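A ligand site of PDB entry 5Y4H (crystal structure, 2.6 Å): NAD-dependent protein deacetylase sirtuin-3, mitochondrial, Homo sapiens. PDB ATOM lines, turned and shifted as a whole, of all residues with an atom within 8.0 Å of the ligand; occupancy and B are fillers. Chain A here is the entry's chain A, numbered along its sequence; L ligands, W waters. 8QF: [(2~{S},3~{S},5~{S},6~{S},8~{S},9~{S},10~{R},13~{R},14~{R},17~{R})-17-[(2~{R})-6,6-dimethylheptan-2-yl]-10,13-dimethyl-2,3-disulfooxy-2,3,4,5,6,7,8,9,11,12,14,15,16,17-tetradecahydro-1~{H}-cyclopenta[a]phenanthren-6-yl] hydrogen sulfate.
The guanidinium group (NH1) of Arg 187 lies within salt-bridge range of an oxygen (O1) of the ligand, at 2.9 Å. N of Gln 186 is in hydrogen-bond range of O9 of the ligand, at 3.0 Å.
Pro 185 touches the ligand. Val 192 touches the ligand (CG1 to C27, 3.8 Å). Val 193 touches the ligand (CG1 to C27, 3.7 Å).
Water W1 lies within hydrogen-bond range of O11 of the ligand (2.7 Å), N of Arg 187 (3.2 Å) and N of Gln 186 (3.4 Å).
The backbone carbonyl oxygen (O) of Ser 128 lies within hydrogen-bond range of the guanidinium group (NH2) of Arg 187, at 3.4 Å. The backbone carbonyl oxygen (O) of Leu 130 lies within hydrogen-bond range of the guanidinium group (NE) of Arg 187 (2.9 Å). The guanidinium group (NH2) of Arg 187 lies within hydrogen-bond range of the backbone carbonyl oxygen (O) of Ala 127 (3.0 Å).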
ATOM      1  N   ALA A 127      -5.213  14.723  28.840  1.00  0.00           N
ATOM      2  CA  ALA A 127      -5.332  13.248  28.772  1.00  0.00           C
ATOM      3  C   ALA A 127      -6.761  12.756  29.028  1.00  0.00           C
ATOM      4  O   ALA A 127      -7.190  11.774  28.410  1.00  0.00           O
ATOM      5  CB  ALA A 127      -4.361  12.562  29.731  1.00  0.00           C
ATOM      6  N   SER A 128      -7.485  13.445  29.906  1.00  0.00           N
ATOM      7  CA  SER A 128      -8.834  13.035  30.301  1.00  0.00           C
ATOM      8  C   SER A 128      -9.893  13.235  29.207  1.00  0.00           C
ATOM      9  O   SER A 128     -10.952  12.593  29.226  1.00  0.00           O
ATOM     10  CB  SER A 128      -9.250  13.760  31.587  1.00  0.00           C
ATOM     11  OG  SER A 128      -9.462  15.126  31.331  1.00  0.00           O
ATOM     12  N   LEU A 130      -9.133  12.674  26.049  1.00  0.00           N
ATOM     13  CA  LEU A 130      -8.545  11.917  24.957  1.00  0.00           C
ATOM     14  C   LEU A 130      -8.697  10.413  25.100  1.00  0.00           C
ATOM     15  O   LEU A 130      -8.612   9.878  26.196  1.00  0.00           O
ATOM     16  CB  LEU A 130      -7.053  12.241  24.865  1.00  0.00           C
ATOM     17  CG  LEU A 130      -6.600  13.259  23.840  1.00  0.00           C
ATOM     18  CD1 LEU A 130      -5.156  13.628  24.140  1.00  0.00           C
ATOM     19  CD2 LEU A 130      -6.750  12.673  22.439  1.00  0.00           C
ATOM     20  N   VAL A 131      -8.933   9.755  23.975  1.00  0.00           N
ATOM     21  CA  VAL A 131      -8.840   8.301  23.875  1.00  0.00           C
ATOM     22  C   VAL A 131      -7.884   8.001  22.702  1.00  0.00           C
ATOM     23  O   VAL A 131      -8.260   8.074  21.523  1.00  0.00           O
ATOM     24  CB  VAL A 131     -10.229   7.613  23.726  1.00  0.00           C
ATOM     25  CG1 VAL A 131     -10.083   6.102  23.558  1.00  0.00           C
ATOM     26  CG2 VAL A 131     -11.123   7.902  24.924  1.00  0.00           C
ATOM     27  N   GLU A 132      -6.645   7.700  23.039  1.00  0.00           N
ATOM     28  CA  GLU A 132      -5.668   7.242  22.057  1.00  0.00           C
ATOM     29  C   GLU A 132      -5.970   5.777  21.728  1.00  0.00           C
ATOM     30  O   GLU A 132      -5.353   4.861  22.276  1.00  0.00           O
ATOM     31  CB  GLU A 132      -4.232   7.469  22.571  1.00  0.00           C
ATOM     32  CG  GLU A 132      -3.790   8.928  22.507  1.00  0.00           C
ATOM     33  CD  GLU A 132      -2.760   9.296  23.554  1.00  0.00           C
ATOM     34  OE1 GLU A 132      -3.127   9.998  24.520  1.00  0.00           O
ATOM     35  OE2 GLU A 132      -1.584   8.898  23.416  1.00  0.00           O
ATOM     36  N   THR A 136      -0.050   4.101  22.228  1.00  0.00           N
ATOM     37  CA  THR A 136       0.818   5.205  22.618  1.00  0.00           C
ATOM     38  C   THR A 136       2.263   4.746  22.746  1.00  0.00           C
ATOM     39  O   THR A 136       2.534   3.574  23.024  1.00  0.00           O
ATOM     40  CB  THR A 136       0.350   5.848  23.949  1.00  0.00           C
ATOM     41  OG1 THR A 136       1.387   6.672  24.466  1.00  0.00           O
ATOM     42  CG2 THR A 136      -0.021   4.784  25.008  1.00  0.00           C
ATOM     43  N   SER A 139       4.615   4.121  26.833  1.00  0.00           N
ATOM     44  CA  SER A 139       5.039   2.889  27.496  1.00  0.00           C
ATOM     45  C   SER A 139       5.273   1.789  26.463  1.00  0.00           C
ATOM     46  O   SER A 139       4.895   1.941  25.289  1.00  0.00           O
ATOM     47  CB  SER A 139       3.999   2.465  28.531  1.00  0.00           C
ATOM     48  OG  SER A 139       2.782   2.142  27.884  1.00  0.00           O
ATOM     49  N   ASP A 176       3.744   0.322  23.158  1.00  0.00           N
ATOM     50  CA  ASP A 176       2.337  -0.093  23.246  1.00  0.00           C
ATOM     51  C   ASP A 176       1.460   0.546  22.166  1.00  0.00           C
ATOM     52  O   ASP A 176       0.511   1.276  22.451  1.00  0.00           O
ATOM     53  CB  ASP A 176       1.767   0.119  24.650  1.00  0.00           C
ATOM     54  CG  ASP A 176       2.465  -0.737  25.693  1.00  0.00           C
ATOM     55  OD1 ASP A 176       3.024  -1.792  25.347  1.00  0.00           O
ATOM     56  OD2 ASP A 176       2.445  -0.337  26.871  1.00  0.00           O
ATOM     57  N   PRO A 183      -6.010  -6.439  20.541  1.00  0.00           N
ATOM     58  CA  PRO A 183      -7.106  -5.682  21.159  1.00  0.00           C
ATOM     59  C   PRO A 183      -6.696  -4.236  21.436  1.00  0.00           C
ATOM     60  O   PRO A 183      -5.513  -3.972  21.701  1.00  0.00           O
ATOM     61  CB  PRO A 183      -7.342  -6.431  22.475  1.00  0.00           C
ATOM     62  CG  PRO A 183      -6.045  -7.093  22.768  1.00  0.00           C
ATOM     63  CD  PRO A 183      -5.519  -7.509  21.428  1.00  0.00           C
ATOM     64  N   LEU A 184      -7.670  -3.333  21.343  1.00  0.00           N
ATOM     65  CA  LEU A 184      -7.442  -1.919  21.608  1.00  0.00           C
ATOM     66  C   LEU A 184      -7.345  -1.721  23.129  1.00  0.00           C
ATOM     67  O   LEU A 184      -7.834  -2.571  23.878  1.00  0.00           O
ATOM     68  CB  LEU A 184      -8.613  -1.062  21.059  1.00  0.00           C
ATOM     69  CG  LEU A 184      -9.215  -1.149  19.650  1.00  0.00           C
ATOM     70  CD1 LEU A 184      -9.663   0.260  19.287  1.00  0.00           C
ATOM     71  CD2 LEU A 184      -8.290  -1.685  18.554  1.00  0.00           C
ATOM     72  N   PRO A 185      -6.712  -0.617  23.586  1.00  0.00           N
ATOM     73  CA  PRO A 185      -6.657  -0.438  25.044  1.00  0.00           C
ATOM     74  C   PRO A 185      -8.056  -0.314  25.642  1.00  0.00           C
ATOM     75  O   PRO A 185      -8.970   0.143  24.979  1.00  0.00           O
ATOM     76  CB  PRO A 185      -5.860   0.856  25.210  1.00  0.00           C
ATOM     77  CG  PRO A 185      -5.961   1.558  23.889  1.00  0.00           C
ATOM     78  CD  PRO A 185      -5.998   0.463  22.882  1.00  0.00           C
ATOM     79  N   GLN A 186      -8.190  -0.713  26.893  1.00  0.00           N
ATOM     80  CA  GLN A 186      -9.478  -0.798  27.575  1.00  0.00           C
ATOM     81  C   GLN A 186     -10.115   0.578  27.831  1.00  0.00           C
ATOM     82  O   GLN A 186     -11.321   0.674  28.073  1.00  0.00           O
ATOM     83  CB  GLN A 186      -9.313  -1.569  28.890  1.00  0.00           C
ATOM     84  CG  GLN A 186      -8.972  -3.042  28.694  1.00  0.00           C
ATOM     85  CD  GLN A 186     -10.148  -3.933  28.986  1.00  0.00           C
ATOM     86  OE1 GLN A 186     -10.410  -4.260  30.140  1.00  0.00           O
ATOM     87  NE2 GLN A 186     -10.888  -4.315  27.948  1.00  0.00           N
ATOM     88  N   ARG A 187      -9.318   1.642  27.754  1.00  0.00           N
ATOM     89  CA  ARG A 187      -9.827   3.015  27.773  1.00  0.00           C
ATOM     90  C   ARG A 187     -10.835   3.291  26.656  1.00  0.00           C
ATOM     91  O   ARG A 187     -11.708   4.163  26.816  1.00  0.00           O
ATOM     92  CB  ARG A 187      -8.693   4.019  27.720  1.00  0.00           C
ATOM     93  CG  ARG A 187      -9.167   5.455  27.926  1.00  0.00           C
ATOM     94  CD  ARG A 187      -8.000   6.402  28.123  1.00  0.00           C
ATOM     95  NE  ARG A 187      -8.429   7.795  28.186  1.00  0.00           N
ATOM     96  CZ  ARG A 187      -8.967   8.393  29.245  1.00  0.00           C
ATOM     97  NH1 ARG A 187      -9.217   7.733  30.368  1.00  0.00           N
ATOM     98  NH2 ARG A 187      -9.279   9.691  29.164  1.00  0.00           N
ATOM     99  N   PHE A 188     -10.713   2.546  25.542  1.00  0.00           N
ATOM    100  CA  PHE A 188     -11.692   2.532  24.445  1.00  0.00           C
ATOM    101  C   PHE A 188     -13.145   2.396  24.935  1.00  0.00           C
ATOM    102  O   PHE A 188     -14.050   2.932  24.296  1.00  0.00           O
ATOM    103  CB  PHE A 188     -11.389   1.400  23.459  1.00  0.00           C
ATOM    104  CG  PHE A 188     -12.101   1.524  22.140  1.00  0.00           C
ATOM    105  CD1 PHE A 188     -11.833   2.598  21.260  1.00  0.00           C
ATOM    106  CD2 PHE A 188     -13.047   0.568  21.743  1.00  0.00           C
ATOM    107  CE1 PHE A 188     -12.503   2.708  20.036  1.00  0.00           C
ATOM    108  CE2 PHE A 188     -13.713   0.673  20.527  1.00  0.00           C
ATOM    109  CZ  PHE A 188     -13.432   1.748  19.666  1.00  0.00           C
ATOM    110  N   LEU A 189     -13.341   1.681  26.052  1.00  0.00           N
ATOM    111  CA  LEU A 189     -14.674   1.435  26.623  1.00  0.00           C
ATOM    112  C   LEU A 189     -15.394   2.700  27.097  1.00  0.00           C
ATOM    113  O   LEU A 189     -16.616   2.679  27.298  1.00  0.00           O
ATOM    114  CB  LEU A 189     -14.636   0.347  27.713  1.00  0.00           C
ATOM    115  CG  LEU A 189     -14.182  -1.070  27.293  1.00  0.00           C
ATOM    116  CD1 LEU A 189     -13.967  -1.927  28.526  1.00  0.00           C
ATOM    117  CD2 LEU A 189     -15.122  -1.784  26.328  1.00  0.00           C
ATOM    118  N   LEU A 190     -14.660   3.810  27.211  1.00  0.00           N
ATOM    119  CA  LEU A 190     -15.286   5.131  27.446  1.00  0.00           C
ATOM    120  C   LEU A 190     -16.318   5.488  26.358  1.00  0.00           C
ATOM    121  O   LEU A 190     -17.215   6.288  26.603  1.00  0.00           O
ATOM    122  CB  LEU A 190     -14.230   6.241  27.597  1.00  0.00           C
ATOM    123  CG  LEU A 190     -13.565   6.437  28.970  1.00  0.00           C
ATOM    124  CD1 LEU A 190     -12.508   7.544  28.948  1.00  0.00           C
ATOM    125  CD2 LEU A 190     -14.575   6.698  30.088  1.00  0.00           C
ATOM    126  N   HIS A 191     -16.191   4.898  25.174  1.00  0.00           N
ATOM    127  CA  HIS A 191     -17.145   5.119  24.088  1.00  0.00           C
ATOM    128  C   HIS A 191     -18.579   4.726  24.435  1.00  0.00           C
ATOM    129  O   HIS A 191     -19.508   5.309  23.894  1.00  0.00           O
ATOM    130  CB  HIS A 191     -16.674   4.452  22.793  1.00  0.00           C
ATOM    131  CG  HIS A 191     -17.115   3.023  22.613  1.00  0.00           C
ATOM    132  ND1 HIS A 191     -16.246   1.959  22.675  1.00  0.00           N
ATOM    133  CD2 HIS A 191     -18.334   2.491  22.313  1.00  0.00           C
ATOM    134  CE1 HIS A 191     -16.896   0.835  22.450  1.00  0.00           C
ATOM    135  NE2 HIS A 191     -18.166   1.127  22.223  1.00  0.00           N
ATOM    136  N   VAL A 192     -18.745   3.751  25.328  1.00  0.00           N
ATOM    137  CA  VAL A 192     -20.067   3.276  25.750  1.00  0.00           C
ATOM    138  C   VAL A 192     -20.850   4.414  26.423  1.00  0.00           C
ATOM    139  O   VAL A 192     -22.050   4.514  26.245  1.00  0.00           O
ATOM    140  CB  VAL A 192     -20.004   2.020  26.654  1.00  0.00           C
ATOM    141  CG1 VAL A 192     -21.386   1.449  26.920  1.00  0.00           C
ATOM    142  CG2 VAL A 192     -19.150   0.936  25.999  1.00  0.00           C
ATOM    143  N   VAL A 193     -20.159   5.282  27.159  1.00  0.00           N
ATOM    144  CA  VAL A 193     -20.818   6.411  27.840  1.00  0.00           C
ATOM    145  C   VAL A 193     -20.725   7.753  27.100  1.00  0.00           C
ATOM    146  O   VAL A 193     -21.625   8.584  27.252  1.00  0.00           O
ATOM    147  CB  VAL A 193     -20.425   6.573  29.330  1.00  0.00           C
ATOM    148  CG1 VAL A 193     -20.826   5.342  30.133  1.00  0.00           C
ATOM    149  CG2 VAL A 193     -18.944   6.908  29.508  1.00  0.00           C
ATOM    150  N   ASP A 194     -19.659   7.949  26.328  1.00  0.00           N
ATOM    151  CA  ASP A 194     -19.475   9.175  25.545  1.00  0.00           C
ATOM    152  C   ASP A 194     -20.440   9.289  24.346  1.00  0.00           C
ATOM    153  O   ASP A 194     -21.131  10.309  24.222  1.00  0.00           O
ATOM    154  CB  ASP A 194     -18.030   9.300  25.065  1.00  0.00           C
ATOM    155  CG  ASP A 194     -17.080   9.743  26.166  1.00  0.00           C
ATOM    156  OD1 ASP A 194     -17.534  10.309  27.179  1.00  0.00           O
ATOM    157  OD2 ASP A 194     -15.861   9.523  26.013  1.00  0.00           O
HETATM  158  C1  8QF L   1     -15.865   0.515  32.376  1.00  0.00           C
HETATM  159  C2  8QF L   1     -14.493   0.969  31.809  1.00  0.00           C
HETATM  160  C3  8QF L   1     -14.431   2.402  31.255  1.00  0.00           C
HETATM  161  O1  8QF L   1      -7.805   5.450  31.399  1.00  0.00           O
HETATM  162  C4  8QF L   1     -12.935   2.715  31.155  1.00  0.00           C
HETATM  163  O2  8QF L   1      -5.719   4.794  30.231  1.00  0.00           O
HETATM  164  O3  8QF L   1      -6.252   4.243  32.660  1.00  0.00           O
HETATM  165  O4  8QF L   1      -6.358  -1.814  33.947  1.00  0.00           O
HETATM  166  C5  8QF L   1     -12.285   1.967  32.316  1.00  0.00           C
HETATM  167  C6  8QF L   1     -13.233   0.807  32.688  1.00  0.00           C
HETATM  168  C7  8QF L   1     -13.484   0.918  34.201  1.00  0.00           C
HETATM  169  O5  8QF L   1      -4.921  -2.673  35.705  1.00  0.00           O
HETATM  170  C8  8QF L   1     -12.643  -0.570  32.319  1.00  0.00           C
HETATM  171  C9  8QF L   1     -11.228  -0.835  32.809  1.00  0.00           C
HETATM  172  C10 8QF L   1     -10.249   0.185  32.226  1.00  0.00           C
HETATM  173  C11 8QF L   1     -10.739   1.664  32.314  1.00  0.00           C
HETATM  174  O6  8QF L   1      -3.925  -2.520  33.418  1.00  0.00           O
HETATM  175  O7  8QF L   1      -5.716  -4.153  34.098  1.00  0.00           O
HETATM  176  O11 8QF L   1      -4.370  -0.242  29.085  1.00  0.00           O
HETATM  177  S2  8QF L   1      -5.162  -1.399  29.381  1.00  0.00           S
HETATM  178  O9  8QF L   1      -5.769  -1.886  28.173  1.00  0.00           O
HETATM  179  O10 8QF L   1      -4.207  -2.587  29.977  1.00  0.00           O
HETATM  180  O8  8QF L   1      -6.258  -1.069  30.392  1.00  0.00           O
HETATM  181  C19 8QF L   1      -6.022  -0.734  31.755  1.00  0.00           C
HETATM  182  C20 8QF L   1      -6.401   0.731  32.028  1.00  0.00           C
HETATM  183  C14 8QF L   1      -7.924   0.939  31.870  1.00  0.00           C
HETATM  184  C13 8QF L   1      -8.358   2.414  31.855  1.00  0.00           C
HETATM  185  O   8QF L   1      -7.492   3.085  30.949  1.00  0.00           O
HETATM  186  S   8QF L   1      -6.839   4.399  31.358  1.00  0.00           S
HETATM  187  C12 8QF L   1      -9.844   2.572  31.444  1.00  0.00           C
HETATM  188  C18 8QF L   1      -6.844  -1.720  32.599  1.00  0.00           C
HETATM  189  S1  8QF L   1      -5.248  -2.815  34.316  1.00  0.00           S
HETATM  190  C17 8QF L   1      -8.357  -1.431  32.601  1.00  0.00           C
HETATM  191  C15 8QF L   1      -8.807   0.037  32.775  1.00  0.00           C
HETATM  192  C16 8QF L   1      -8.690   0.420  34.259  1.00  0.00           C
HETATM  193  C   8QF L   1     -15.953  -1.005  32.590  1.00  0.00           C
HETATM  194  C21 8QF L   1     -17.054   0.910  31.522  1.00  0.00           C
HETATM  195  C22 8QF L   1     -18.167   1.534  32.338  1.00  0.00           C
HETATM  196  C23 8QF L   1     -19.312   1.988  31.418  1.00  0.00           C
HETATM  197  C24 8QF L   1     -20.732   1.691  31.907  1.00  0.00           C
HETATM  198  C27 8QF L   1     -21.685   1.819  30.722  1.00  0.00           C
HETATM  199  C26 8QF L   1     -20.924   0.263  32.442  1.00  0.00           C
HETATM  200  C25 8QF L   1     -21.108   2.730  32.966  1.00  0.00           C
HETATM  201  O   HOH W   1      -6.208   1.583  28.508  1.00  0.00           O
